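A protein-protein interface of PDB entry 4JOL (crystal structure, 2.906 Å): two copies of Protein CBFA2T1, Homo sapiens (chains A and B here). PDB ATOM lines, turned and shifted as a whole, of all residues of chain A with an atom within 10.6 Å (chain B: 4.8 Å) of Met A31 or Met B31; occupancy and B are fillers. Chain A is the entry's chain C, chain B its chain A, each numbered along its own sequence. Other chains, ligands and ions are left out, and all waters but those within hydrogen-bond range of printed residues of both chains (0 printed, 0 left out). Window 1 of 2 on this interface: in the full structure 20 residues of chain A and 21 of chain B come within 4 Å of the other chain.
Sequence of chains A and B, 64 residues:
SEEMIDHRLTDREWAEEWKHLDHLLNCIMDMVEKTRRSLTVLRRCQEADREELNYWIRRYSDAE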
ATOM      1  N   HIS A  20      -6.873  23.087 -13.601  1.00  0.00           N
ATOM      2  CA  HIS A  20      -5.762  23.669 -14.333  1.00  0.00           C
ATOM      3  C   HIS A  20      -4.721  24.323 -13.427  1.00  0.00           C
ATOM      4  O   HIS A  20      -3.524  24.160 -13.654  1.00  0.00           O
ATOM      5  CB  HIS A  20      -6.213  24.626 -15.431  1.00  0.00           C
ATOM      6  CG  HIS A  20      -5.236  24.714 -16.559  1.00  0.00           C
ATOM      7  ND1 HIS A  20      -4.118  25.520 -16.515  1.00  0.00           N
ATOM      8  CD2 HIS A  20      -5.175  24.052 -17.738  1.00  0.00           C
ATOM      9  CE1 HIS A  20      -3.424  25.371 -17.627  1.00  0.00           C
ATOM     10  NE2 HIS A  20      -4.043  24.485 -18.387  1.00  0.00           N
ATOM     11  N   LEU A  21      -5.164  25.063 -12.414  1.00  0.00           N
ATOM     12  CA  LEU A  21      -4.247  25.534 -11.373  1.00  0.00           C
ATOM     13  C   LEU A  21      -3.444  24.376 -10.798  1.00  0.00           C
ATOM     14  O   LEU A  21      -2.230  24.490 -10.606  1.00  0.00           O
ATOM     15  CB  LEU A  21      -4.993  26.214 -10.222  1.00  0.00           C
ATOM     16  CG  LEU A  21      -5.179  27.726 -10.308  1.00  0.00           C
ATOM     17  CD1 LEU A  21      -6.008  28.209  -9.144  1.00  0.00           C
ATOM     18  CD2 LEU A  21      -3.848  28.454 -10.381  1.00  0.00           C
ATOM     19  N   ASP A  22      -4.119  23.267 -10.497  1.00  0.00           N
ATOM     20  CA  ASP A  22      -3.399  22.152  -9.913  1.00  0.00           C
ATOM     21  C   ASP A  22      -2.262  21.772 -10.815  1.00  0.00           C
ATOM     22  O   ASP A  22      -1.132  21.629 -10.379  1.00  0.00           O
ATOM     23  CB  ASP A  22      -4.271  20.930  -9.697  1.00  0.00           C
ATOM     24  CG  ASP A  22      -3.723  20.046  -8.594  1.00  0.00           C
ATOM     25  OD1 ASP A  22      -3.513  18.829  -8.823  1.00  0.00           O
ATOM     26  OD2 ASP A  22      -3.487  20.602  -7.487  1.00  0.00           O
ATOM     27  N   HIS A  23      -2.581  21.626 -12.091  1.00  0.00           N
ATOM     28  CA  HIS A  23      -1.605  21.240 -13.081  1.00  0.00           C
ATOM     29  C   HIS A  23      -0.424  22.211 -13.195  1.00  0.00           C
ATOM     30  O   HIS A  23       0.725  21.787 -13.241  1.00  0.00           O
ATOM     31  CB  HIS A  23      -2.285  21.105 -14.419  1.00  0.00           C
ATOM     32  CG  HIS A  23      -1.360  20.667 -15.499  1.00  0.00           C
ATOM     33  ND1 HIS A  23      -0.713  19.452 -15.467  1.00  0.00           N
ATOM     34  CD2 HIS A  23      -0.951  21.289 -16.629  1.00  0.00           C
ATOM     35  CE1 HIS A  23       0.042  19.337 -16.545  1.00  0.00           C
ATOM     36  NE2 HIS A  23      -0.085  20.438 -17.266  1.00  0.00           N
ATOM     37  N   LEU A  24      -0.705  23.507 -13.248  1.00  0.00           N
ATOM     38  CA  LEU A  24       0.355  24.510 -13.274  1.00  0.00           C
ATOM     39  C   LEU A  24       1.331  24.305 -12.115  1.00  0.00           C
ATOM     40  O   LEU A  24       2.552  24.313 -12.298  1.00  0.00           O
ATOM     41  CB  LEU A  24      -0.239  25.922 -13.195  1.00  0.00           C
ATOM     42  CG  LEU A  24      -0.619  26.672 -14.475  1.00  0.00           C
ATOM     43  CD1 LEU A  24      -0.041  25.986 -15.697  1.00  0.00           C
ATOM     44  CD2 LEU A  24      -2.119  26.803 -14.601  1.00  0.00           C
ATOM     45  N   LEU A  25       0.783  24.130 -10.917  1.00  0.00           N
ATOM     46  CA  LEU A  25       1.595  23.989  -9.717  1.00  0.00           C
ATOM     47  C   LEU A  25       2.407  22.708  -9.760  1.00  0.00           C
ATOM     48  O   LEU A  25       3.575  22.690  -9.373  1.00  0.00           O
ATOM     49  CB  LEU A  25       0.728  24.047  -8.458  1.00  0.00           C
ATOM     50  CG  LEU A  25       0.140  25.439  -8.201  1.00  0.00           C
ATOM     51  CD1 LEU A  25      -0.574  25.485  -6.855  1.00  0.00           C
ATOM     52  CD2 LEU A  25       1.234  26.516  -8.289  1.00  0.00           C
ATOM     53  N   ASN A  26       1.791  21.639 -10.244  1.00  0.00           N
ATOM     54  CA  ASN A  26       2.492  20.373 -10.373  1.00  0.00           C
ATOM     55  C   ASN A  26       3.645  20.485 -11.350  1.00  0.00           C
ATOM     56  O   ASN A  26       4.734  20.008 -11.056  1.00  0.00           O
ATOM     57  CB  ASN A  26       1.540  19.222 -10.736  1.00  0.00           C
ATOM     58  CG  ASN A  26       0.667  18.785  -9.549  1.00  0.00           C
ATOM     59  OD1 ASN A  26       1.130  18.714  -8.407  1.00  0.00           O
ATOM     60  ND2 ASN A  26      -0.605  18.511  -9.820  1.00  0.00           N
ATOM     61  N   CYS A  27       3.425  21.133 -12.496  1.00  0.00           N
ATOM     62  CA  CYS A  27       4.519  21.371 -13.451  1.00  0.00           C
ATOM     63  C   CYS A  27       5.679  22.095 -12.787  1.00  0.00           C
ATOM     64  O   CYS A  27       6.843  21.709 -12.918  1.00  0.00           O
ATOM     65  CB  CYS A  27       4.058  22.169 -14.670  1.00  0.00           C
ATOM     66  SG  CYS A  27       2.904  21.280 -15.786  1.00  0.00           S
ATOM     67  N   ILE A  28       5.350  23.152 -12.062  1.00  0.00           N
ATOM     68  CA  ILE A  28       6.355  23.906 -11.342  1.00  0.00           C
ATOM     69  C   ILE A  28       7.169  23.020 -10.395  1.00  0.00           C
ATOM     70  O   ILE A  28       8.400  23.045 -10.418  1.00  0.00           O
ATOM     71  CB  ILE A  28       5.703  25.064 -10.614  1.00  0.00           C
ATOM     72  CG1 ILE A  28       5.129  26.016 -11.665  1.00  0.00           C
ATOM     73  CG2 ILE A  28       6.697  25.751  -9.677  1.00  0.00           C
ATOM     74  CD1 ILE A  28       4.391  27.166 -11.093  1.00  0.00           C
ATOM     75  N   MET A  29       6.495  22.213  -9.585  1.00  0.00           N
ATOM     76  CA  MET A  29       7.214  21.286  -8.722  1.00  0.00           C
ATOM     77  C   MET A  29       8.083  20.350  -9.544  1.00  0.00           C
ATOM     78  O   MET A  29       9.229  20.066  -9.193  1.00  0.00           O
ATOM     79  CB  MET A  29       6.252  20.453  -7.899  1.00  0.00           C
ATOM     80  CG  MET A  29       5.089  21.221  -7.362  1.00  0.00           C
ATOM     81  SD  MET A  29       4.691  20.557  -5.763  1.00  0.00           S
ATOM     82  CE  MET A  29       6.255  20.904  -4.976  1.00  0.00           C
ATOM     83  N   ASP A  30       7.532  19.865 -10.645  1.00  0.00           N
ATOM     84  CA  ASP A  30       8.234  18.879 -11.437  1.00  0.00           C
ATOM     85  C   ASP A  30       9.490  19.512 -12.012  1.00  0.00           C
ATOM     86  O   ASP A  30      10.550  18.887 -12.045  1.00  0.00           O
ATOM     87  CB  ASP A  30       7.330  18.315 -12.535  1.00  0.00           C
ATOM     88  CG  ASP A  30       7.993  17.196 -13.313  1.00  0.00           C
ATOM     89  OD1 ASP A  30       8.182  16.098 -12.730  1.00  0.00           O
ATOM     90  OD2 ASP A  30       8.334  17.426 -14.499  1.00  0.00           O
ATOM     91  N   MET A  31       9.379  20.765 -12.439  1.00  0.00           N
ATOM     92  CA  MET A  31      10.536  21.461 -12.983  1.00  0.00           C
ATOM     93  C   MET A  31      11.584  21.657 -11.892  1.00  0.00           C
ATOM     94  O   MET A  31      12.769  21.411 -12.108  1.00  0.00           O
ATOM     95  CB  MET A  31      10.130  22.802 -13.598  1.00  0.00           C
ATOM     96  CG  MET A  31      10.638  22.987 -15.032  1.00  0.00           C
ATOM     97  SD  MET A  31      10.176  24.552 -15.781  1.00  0.00           S
ATOM     98  CE  MET A  31       8.436  24.670 -15.316  1.00  0.00           C
ATOM     99  N   VAL A  32      11.134  22.081 -10.716  1.00  0.00           N
ATOM    100  CA  VAL A  32      12.034  22.334  -9.602  1.00  0.00           C
ATOM    101  C   VAL A  32      12.720  21.050  -9.177  1.00  0.00           C
ATOM    102  O   VAL A  32      13.912  21.050  -8.906  1.00  0.00           O
ATOM    103  CB  VAL A  32      11.301  22.963  -8.385  1.00  0.00           C
ATOM    104  CG1 VAL A  32      12.277  23.206  -7.233  1.00  0.00           C
ATOM    105  CG2 VAL A  32      10.625  24.267  -8.782  1.00  0.00           C
ATOM    106  N   GLU A  33      11.965  19.955  -9.127  1.00  0.00           N
ATOM    107  CA  GLU A  33      12.511  18.675  -8.672  1.00  0.00           C
ATOM    108  C   GLU A  33      13.539  18.130  -9.660  1.00  0.00           C
ATOM    109  O   GLU A  33      14.604  17.647  -9.262  1.00  0.00           O
ATOM    110  CB  GLU A  33      11.391  17.649  -8.422  1.00  0.00           C
ATOM    111  CG  GLU A  33      11.860  16.216  -8.117  1.00  0.00           C
ATOM    112  CD  GLU A  33      12.630  16.086  -6.806  1.00  0.00           C
ATOM    113  OE1 GLU A  33      12.616  17.041  -5.995  1.00  0.00           O
ATOM    114  OE2 GLU A  33      13.245  15.019  -6.586  1.00  0.00           O
ATOM    115  N   LYS A  34      13.230  18.215 -10.948  1.00  0.00           N
ATOM    116  CA  LYS A  34      14.191  17.791 -11.956  1.00  0.00           C
ATOM    117  C   LYS A  34      15.437  18.663 -11.886  1.00  0.00           C
ATOM    118  O   LYS A  34      16.553  18.159 -11.962  1.00  0.00           O
ATOM    119  CB  LYS A  34      13.561  17.753 -13.352  1.00  0.00           C
ATOM    120  CG  LYS A  34      12.568  16.617 -13.454  1.00  0.00           C
ATOM    121  CD  LYS A  34      11.902  16.501 -14.797  1.00  0.00           C
ATOM    122  CE  LYS A  34      10.903  15.360 -14.750  1.00  0.00           C
ATOM    123  NZ  LYS A  34       9.994  15.367 -15.926  1.00  0.00           N
ATOM    124  N   THR A  35      15.236  19.962 -11.693  1.00  0.00           N
ATOM    125  CA  THR A  35      16.343  20.895 -11.514  1.00  0.00           C
ATOM    126  C   THR A  35      17.235  20.530 -10.315  1.00  0.00           C
ATOM    127  O   THR A  35      18.470  20.490 -10.426  1.00  0.00           O
ATOM    128  CB  THR A  35      15.835  22.336 -11.388  1.00  0.00           C
ATOM    129  OG1 THR A  35      15.333  22.771 -12.660  1.00  0.00           O
ATOM    130  CG2 THR A  35      16.967  23.250 -10.972  1.00  0.00           C
ATOM    131  N   ARG A  36      16.592  20.252  -9.187  1.00  0.00           N
ATOM    132  CA  ARG A  36      17.260  19.842  -7.964  1.00  0.00           C
ATOM    133  C   ARG A  36      18.187  18.646  -8.173  1.00  0.00           C
ATOM    134  O   ARG A  36      19.359  18.678  -7.775  1.00  0.00           O
ATOM    135  CB  ARG A  36      16.215  19.484  -6.908  1.00  0.00           C
ATOM    136  CG  ARG A  36      16.574  19.915  -5.497  1.00  0.00           C
ATOM    137  CD  ARG A  36      15.695  19.218  -4.491  1.00  0.00           C
ATOM    138  NE  ARG A  36      15.704  17.774  -4.704  1.00  0.00           N
ATOM    139  CZ  ARG A  36      15.864  16.876  -3.737  1.00  0.00           C
ATOM    140  NH1 ARG A  36      16.026  17.272  -2.478  1.00  0.00           N
ATOM    141  NH2 ARG A  36      15.859  15.581  -4.025  1.00  0.00           N
ATOM    142  N   ARG A  37      17.655  17.587  -8.779  1.00  0.00           N
ATOM    143  CA  ARG A  37      18.420  16.362  -8.989  1.00  0.00           C
ATOM    144  C   ARG A  37      19.588  16.673  -9.892  1.00  0.00           C
ATOM    145  O   ARG A  37      20.700  16.152  -9.708  1.00  0.00           O
ATOM    146  CB  ARG A  37      17.557  15.284  -9.646  1.00  0.00           C
ATOM    147  CG  ARG A  37      16.398  14.816  -8.808  1.00  0.00           C
ATOM    148  CD  ARG A  37      16.382  13.304  -8.670  1.00  0.00           C
ATOM    149  NE  ARG A  37      15.204  12.882  -7.924  1.00  0.00           N
ATOM    150  CZ  ARG A  37      13.968  12.906  -8.414  1.00  0.00           C
ATOM    151  NH1 ARG A  37      13.757  13.328  -9.654  1.00  0.00           N
ATOM    152  NH2 ARG A  37      12.947  12.514  -7.665  1.00  0.00           N
ATOM    153  N   SER A  38      19.304  17.527 -10.873  1.00  0.00           N
ATOM    154  CA  SER A  38      20.268  17.960 -11.865  1.00  0.00           C
ATOM    155  C   SER A  38      21.549  18.431 -11.181  1.00  0.00           C
ATOM    156  O   SER A  38      22.670  18.089 -11.596  1.00  0.00           O
ATOM    157  CB  SER A  38      19.645  19.086 -12.679  1.00  0.00           C
ATOM    158  OG  SER A  38      20.597  19.721 -13.494  1.00  0.00           O
ATOM    159  N   LEU A  39      21.367  19.206 -10.114  1.00  0.00           N
ATOM    160  CA  LEU A  39      22.484  19.748  -9.345  1.00  0.00           C
ATOM    161  C   LEU A  39      23.290  18.663  -8.621  1.00  0.00           C
ATOM    162  O   LEU A  39      24.478  18.838  -8.347  1.00  0.00           O
ATOM    163  CB  LEU A  39      21.983  20.808  -8.360  1.00  0.00           C
ATOM    164  CG  LEU A  39      21.328  22.027  -9.017  1.00  0.00           C
ATOM    165  CD1 LEU A  39      20.797  23.001  -7.983  1.00  0.00           C
ATOM    166  CD2 LEU A  39      22.281  22.726  -9.968  1.00  0.00           C
ATOM    167  N   LEU B  24      15.999  27.102 -16.960  1.00  0.00           N
ATOM    168  CA  LEU B  24      15.051  26.384 -16.125  1.00  0.00           C
ATOM    169  C   LEU B  24      14.473  27.344 -15.094  1.00  0.00           C
ATOM    170  O   LEU B  24      13.259  27.508 -15.000  1.00  0.00           O
ATOM    171  CB  LEU B  24      15.715  25.197 -15.430  1.00  0.00           C
ATOM    172  CG  LEU B  24      16.150  24.031 -16.311  1.00  0.00           C
ATOM    173  CD1 LEU B  24      17.093  23.135 -15.561  1.00  0.00           C
ATOM    174  CD2 LEU B  24      14.944  23.245 -16.765  1.00  0.00           C
ATOM    175  N   CYS B  27      12.011  29.705 -16.632  1.00  0.00           N
ATOM    176  CA  CYS B  27      10.750  29.038 -16.918  1.00  0.00           C
ATOM    177  C   CYS B  27       9.890  28.944 -15.659  1.00  0.00           C
ATOM    178  O   CYS B  27       8.690  29.202 -15.691  1.00  0.00           O
ATOM    179  CB  CYS B  27      10.994  27.657 -17.509  1.00  0.00           C
ATOM    180  SG  CYS B  27      11.825  27.688 -19.118  1.00  0.00           S
ATOM    181  N   ILE B  28      10.510  28.589 -14.543  1.00  0.00           N
ATOM    182  CA  ILE B  28       9.804  28.555 -13.270  1.00  0.00           C
ATOM    183  C   ILE B  28       9.215  29.918 -12.898  1.00  0.00           C
ATOM    184  O   ILE B  28       8.019  30.015 -12.619  1.00  0.00           O
ATOM    185  CB  ILE B  28      10.701  28.010 -12.154  1.00  0.00           C
ATOM    186  CG1 ILE B  28      11.146  26.593 -12.525  1.00  0.00           C
ATOM    187  CG2 ILE B  28       9.983  28.056 -10.789  1.00  0.00           C
ATOM    188  CD1 ILE B  28      11.956  25.923 -11.468  1.00  0.00           C
ATOM    189  N   MET B  29      10.044  30.964 -12.914  1.00  0.00           N
ATOM    190  CA  MET B  29       9.579  32.340 -12.669  1.00  0.00           C
ATOM    191  C   MET B  29       8.359  32.657 -13.516  1.00  0.00           C
ATOM    192  O   MET B  29       7.379  33.240 -13.045  1.00  0.00           O
ATOM    193  CB  MET B  29      10.655  33.376 -13.036  1.00  0.00           C
ATOM    194  CG  MET B  29      12.008  33.195 -12.380  1.00  0.00           C
ATOM    195  SD  MET B  29      12.315  34.455 -11.143  1.00  0.00           S
ATOM    196  CE  MET B  29      10.872  34.215 -10.117  1.00  0.00           C
ATOM    197  N   ASP B  30       8.445  32.272 -14.783  1.00  0.00           N
ATOM    198  CA  ASP B  30       7.456  32.652 -15.766  1.00  0.00           C
ATOM    199  C   ASP B  30       6.129  31.962 -15.495  1.00  0.00           C
ATOM    200  O   ASP B  30       5.093  32.620 -15.476  1.00  0.00           O
ATOM    201  CB  ASP B  30       7.965  32.354 -17.180  1.00  0.00           C
ATOM    202  CG  ASP B  30       6.974  32.762 -18.252  1.00  0.00           C
ATOM    203  OD1 ASP B  30       6.897  33.976 -18.558  1.00  0.00           O
ATOM    204  OD2 ASP B  30       6.271  31.864 -18.777  1.00  0.00           O
ATOM    205  N   MET B  31       6.151  30.649 -15.276  1.00  0.00           N
ATOM    206  CA  MET B  31       4.922  29.949 -14.891  1.00  0.00           C
ATOM    207  C   MET B  31       4.304  30.570 -13.642  1.00  0.00           C
ATOM    208  O   MET B  31       3.105  30.830 -13.586  1.00  0.00           O
ATOM    209  CB  MET B  31       5.181  28.474 -14.604  1.00  0.00           C
ATOM    210  CG  MET B  31       5.849  27.707 -15.713  1.00  0.00           C
ATOM    211  SD  MET B  31       5.404  25.982 -15.562  1.00  0.00           S
ATOM    212  CE  MET B  31       3.620  26.158 -15.559  1.00  0.00           C
ATOM    213  N   VAL B  32       5.130  30.796 -12.630  1.00  0.00           N
ATOM    214  CA  VAL B  32       4.619  31.296 -11.375  1.00  0.00           C
ATOM    215  C   VAL B  32       3.932  32.632 -11.603  1.00  0.00           C
ATOM    216  O   VAL B  32       2.792  32.830 -11.176  1.00  0.00           O
ATOM    217  CB  VAL B  32       5.727  31.390 -10.307  1.00  0.00           C
ATOM    218  CG1 VAL B  32       5.186  31.981  -9.015  1.00  0.00           C
ATOM    219  CG2 VAL B  32       6.286  30.003 -10.044  1.00  0.00           C
ATOM    220  N   GLU B  33       4.620  33.525 -12.308  1.00  0.00           N
ATOM    221  CA  GLU B  33       4.126  34.879 -12.549  1.00  0.00           C
ATOM    222  C   GLU B  33       2.828  34.888 -13.350  1.00  0.00           C
ATOM    223  O   GLU B  33       1.905  35.648 -13.057  1.00  0.00           O
ATOM    224  CB  GLU B  33       5.183  35.712 -13.276  1.00  0.00           C
ATOM    225  CG  GLU B  33       4.683  37.071 -13.755  1.00  0.00           C
ATOM    226  CD  GLU B  33       4.289  37.987 -12.612  1.00  0.00           C
ATOM    227  OE1 GLU B  33       4.728  37.736 -11.466  1.00  0.00           O
ATOM    228  OE2 GLU B  33       3.541  38.955 -12.858  1.00  0.00           O
ATOM    229  N   LYS B  34       2.759  34.051 -14.371  1.00  0.00           N
ATOM    230  CA  LYS B  34       1.537  33.937 -15.137  1.00  0.00           C
ATOM    231  C   LYS B  34       0.423  33.432 -14.239  1.00  0.00           C
ATOM    232  O   LYS B  34      -0.683  33.975 -14.234  1.00  0.00           O
ATOM    233  CB  LYS B  34       1.743  33.053 -16.367  1.00  0.00           C
ATOM    234  CG  LYS B  34       2.580  33.764 -17.419  1.00  0.00           C
ATOM    235  CD  LYS B  34       2.840  32.895 -18.633  1.00  0.00           C
ATOM    236  CE  LYS B  34       3.739  33.607 -19.630  1.00  0.00           C
ATOM    237  NZ  LYS B  34       4.208  32.673 -20.697  1.00  0.00           N
ATOM    238  N   THR B  35       0.728  32.414 -13.452  1.00  0.00           N
ATOM    239  CA  THR B  35      -0.236  31.924 -12.483  1.00  0.00           C
ATOM    240  C   THR B  35      -0.730  33.035 -11.539  1.00  0.00           C
ATOM    241  O   THR B  35      -1.935  33.221 -11.358  1.00  0.00           O
ATOM    242  CB  THR B  35       0.328  30.759 -11.709  1.00  0.00           C
ATOM    243  OG1 THR B  35       0.557  29.669 -12.616  1.00  0.00           O
ATOM    244  CG2 THR B  35      -0.654  30.326 -10.656  1.00  0.00           C
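Of the printed residues of chain B, Leu A21 touches Thr B35 (3.7 Å). Printed residues of chain B within 4 Å of Ile A28: Met B31 (3.8 Å) and Val B32 (3.6 Å). Of chain B, only Cys B27 (3.6 Å), Ile B28 (3.96 Å) and Met B31 (3.3 Å) come within 4 Å of Met A31. Of the printed residues of chain B, Val A32 touches Ile B28 (3.4 Å). Of the printed residues of chain B, Thr A35 touches Leu B24. Of the printed residues of chain A, Leu B24 touches Thr A35. Of chain A, only Met A31 (3.6 Å) comes within 4 Å of Cys B27. Of the printed residues of chain A, Ile B28 touches Met A31 and Val A32. Of chain A, only Leu A24, Ile A28 and Met A31 come within 4 Å of Met B31. Val B32 touches just one residue of chain A: Ile A28 (3.6 Å). No residue of chain A comes within 4 Å of Lys B34. Printed residues of chain A within 4 Å of Thr B35: Leu A21 (3.7 Å) and Leu A24 (3.7 Å). The nearest residue of chain A that does not touch Met B31 is Cys A27 (4.1 Å).
Among the printed residues, merely in contact across the chains: Leu A21 with Thr B35, Leu A24 with Met B31, Leu A24 with Thr B35, Ile A28 with Met B31, Ile A28 with Val B32, Met A31 with Cys B27, Met A31 with Ile B28, Met A31 with Met B31, Val A32 with Ile B28 and Thr A35 with Leu B24.
The backbone carbonyl oxygen (O) of Met B31 sits at hydrogen-bond distance from the side-chain hydroxyl (OG1) of Thr B35. The side-chain hydroxyl (OG1) of Thr A35 sits at hydrogen-bond distance from the backbone carbonyl oxygen (O) of Met A31 (3.0 Å).
Leu A24 touches Met B31, but with the chains exchanged Met A31 does not touch Leu B24 (4.3 Å). Leu A24 touches Thr B35, and with the chains exchanged Thr A35 touches Leu B24. Ile A28 touches Met B31, and with the chains exchanged Met A31 touches Ile B28. Met A31 touches its own counterpart, Met B31. 10 positions are printed for both chains. Of the 10 pairs that touch across the chains among the printed residues, 7 have their exchanged pair printed and touching as well.
Hydrophobic or aromatic side chains of chain B within 4 Å of the printed part of chain A: Leu B24, Ile B28, Met B31 and Val B32. Along chain A the printed residues that touch a printed residue of chain B span positions 21 to 35. Among the printed residues, 10 pairs touch across the chains. Among the printed residues, no Asp or Glu carboxylate lies within 4 Å of a Lys or Arg side-chain nitrogen of the other chain.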
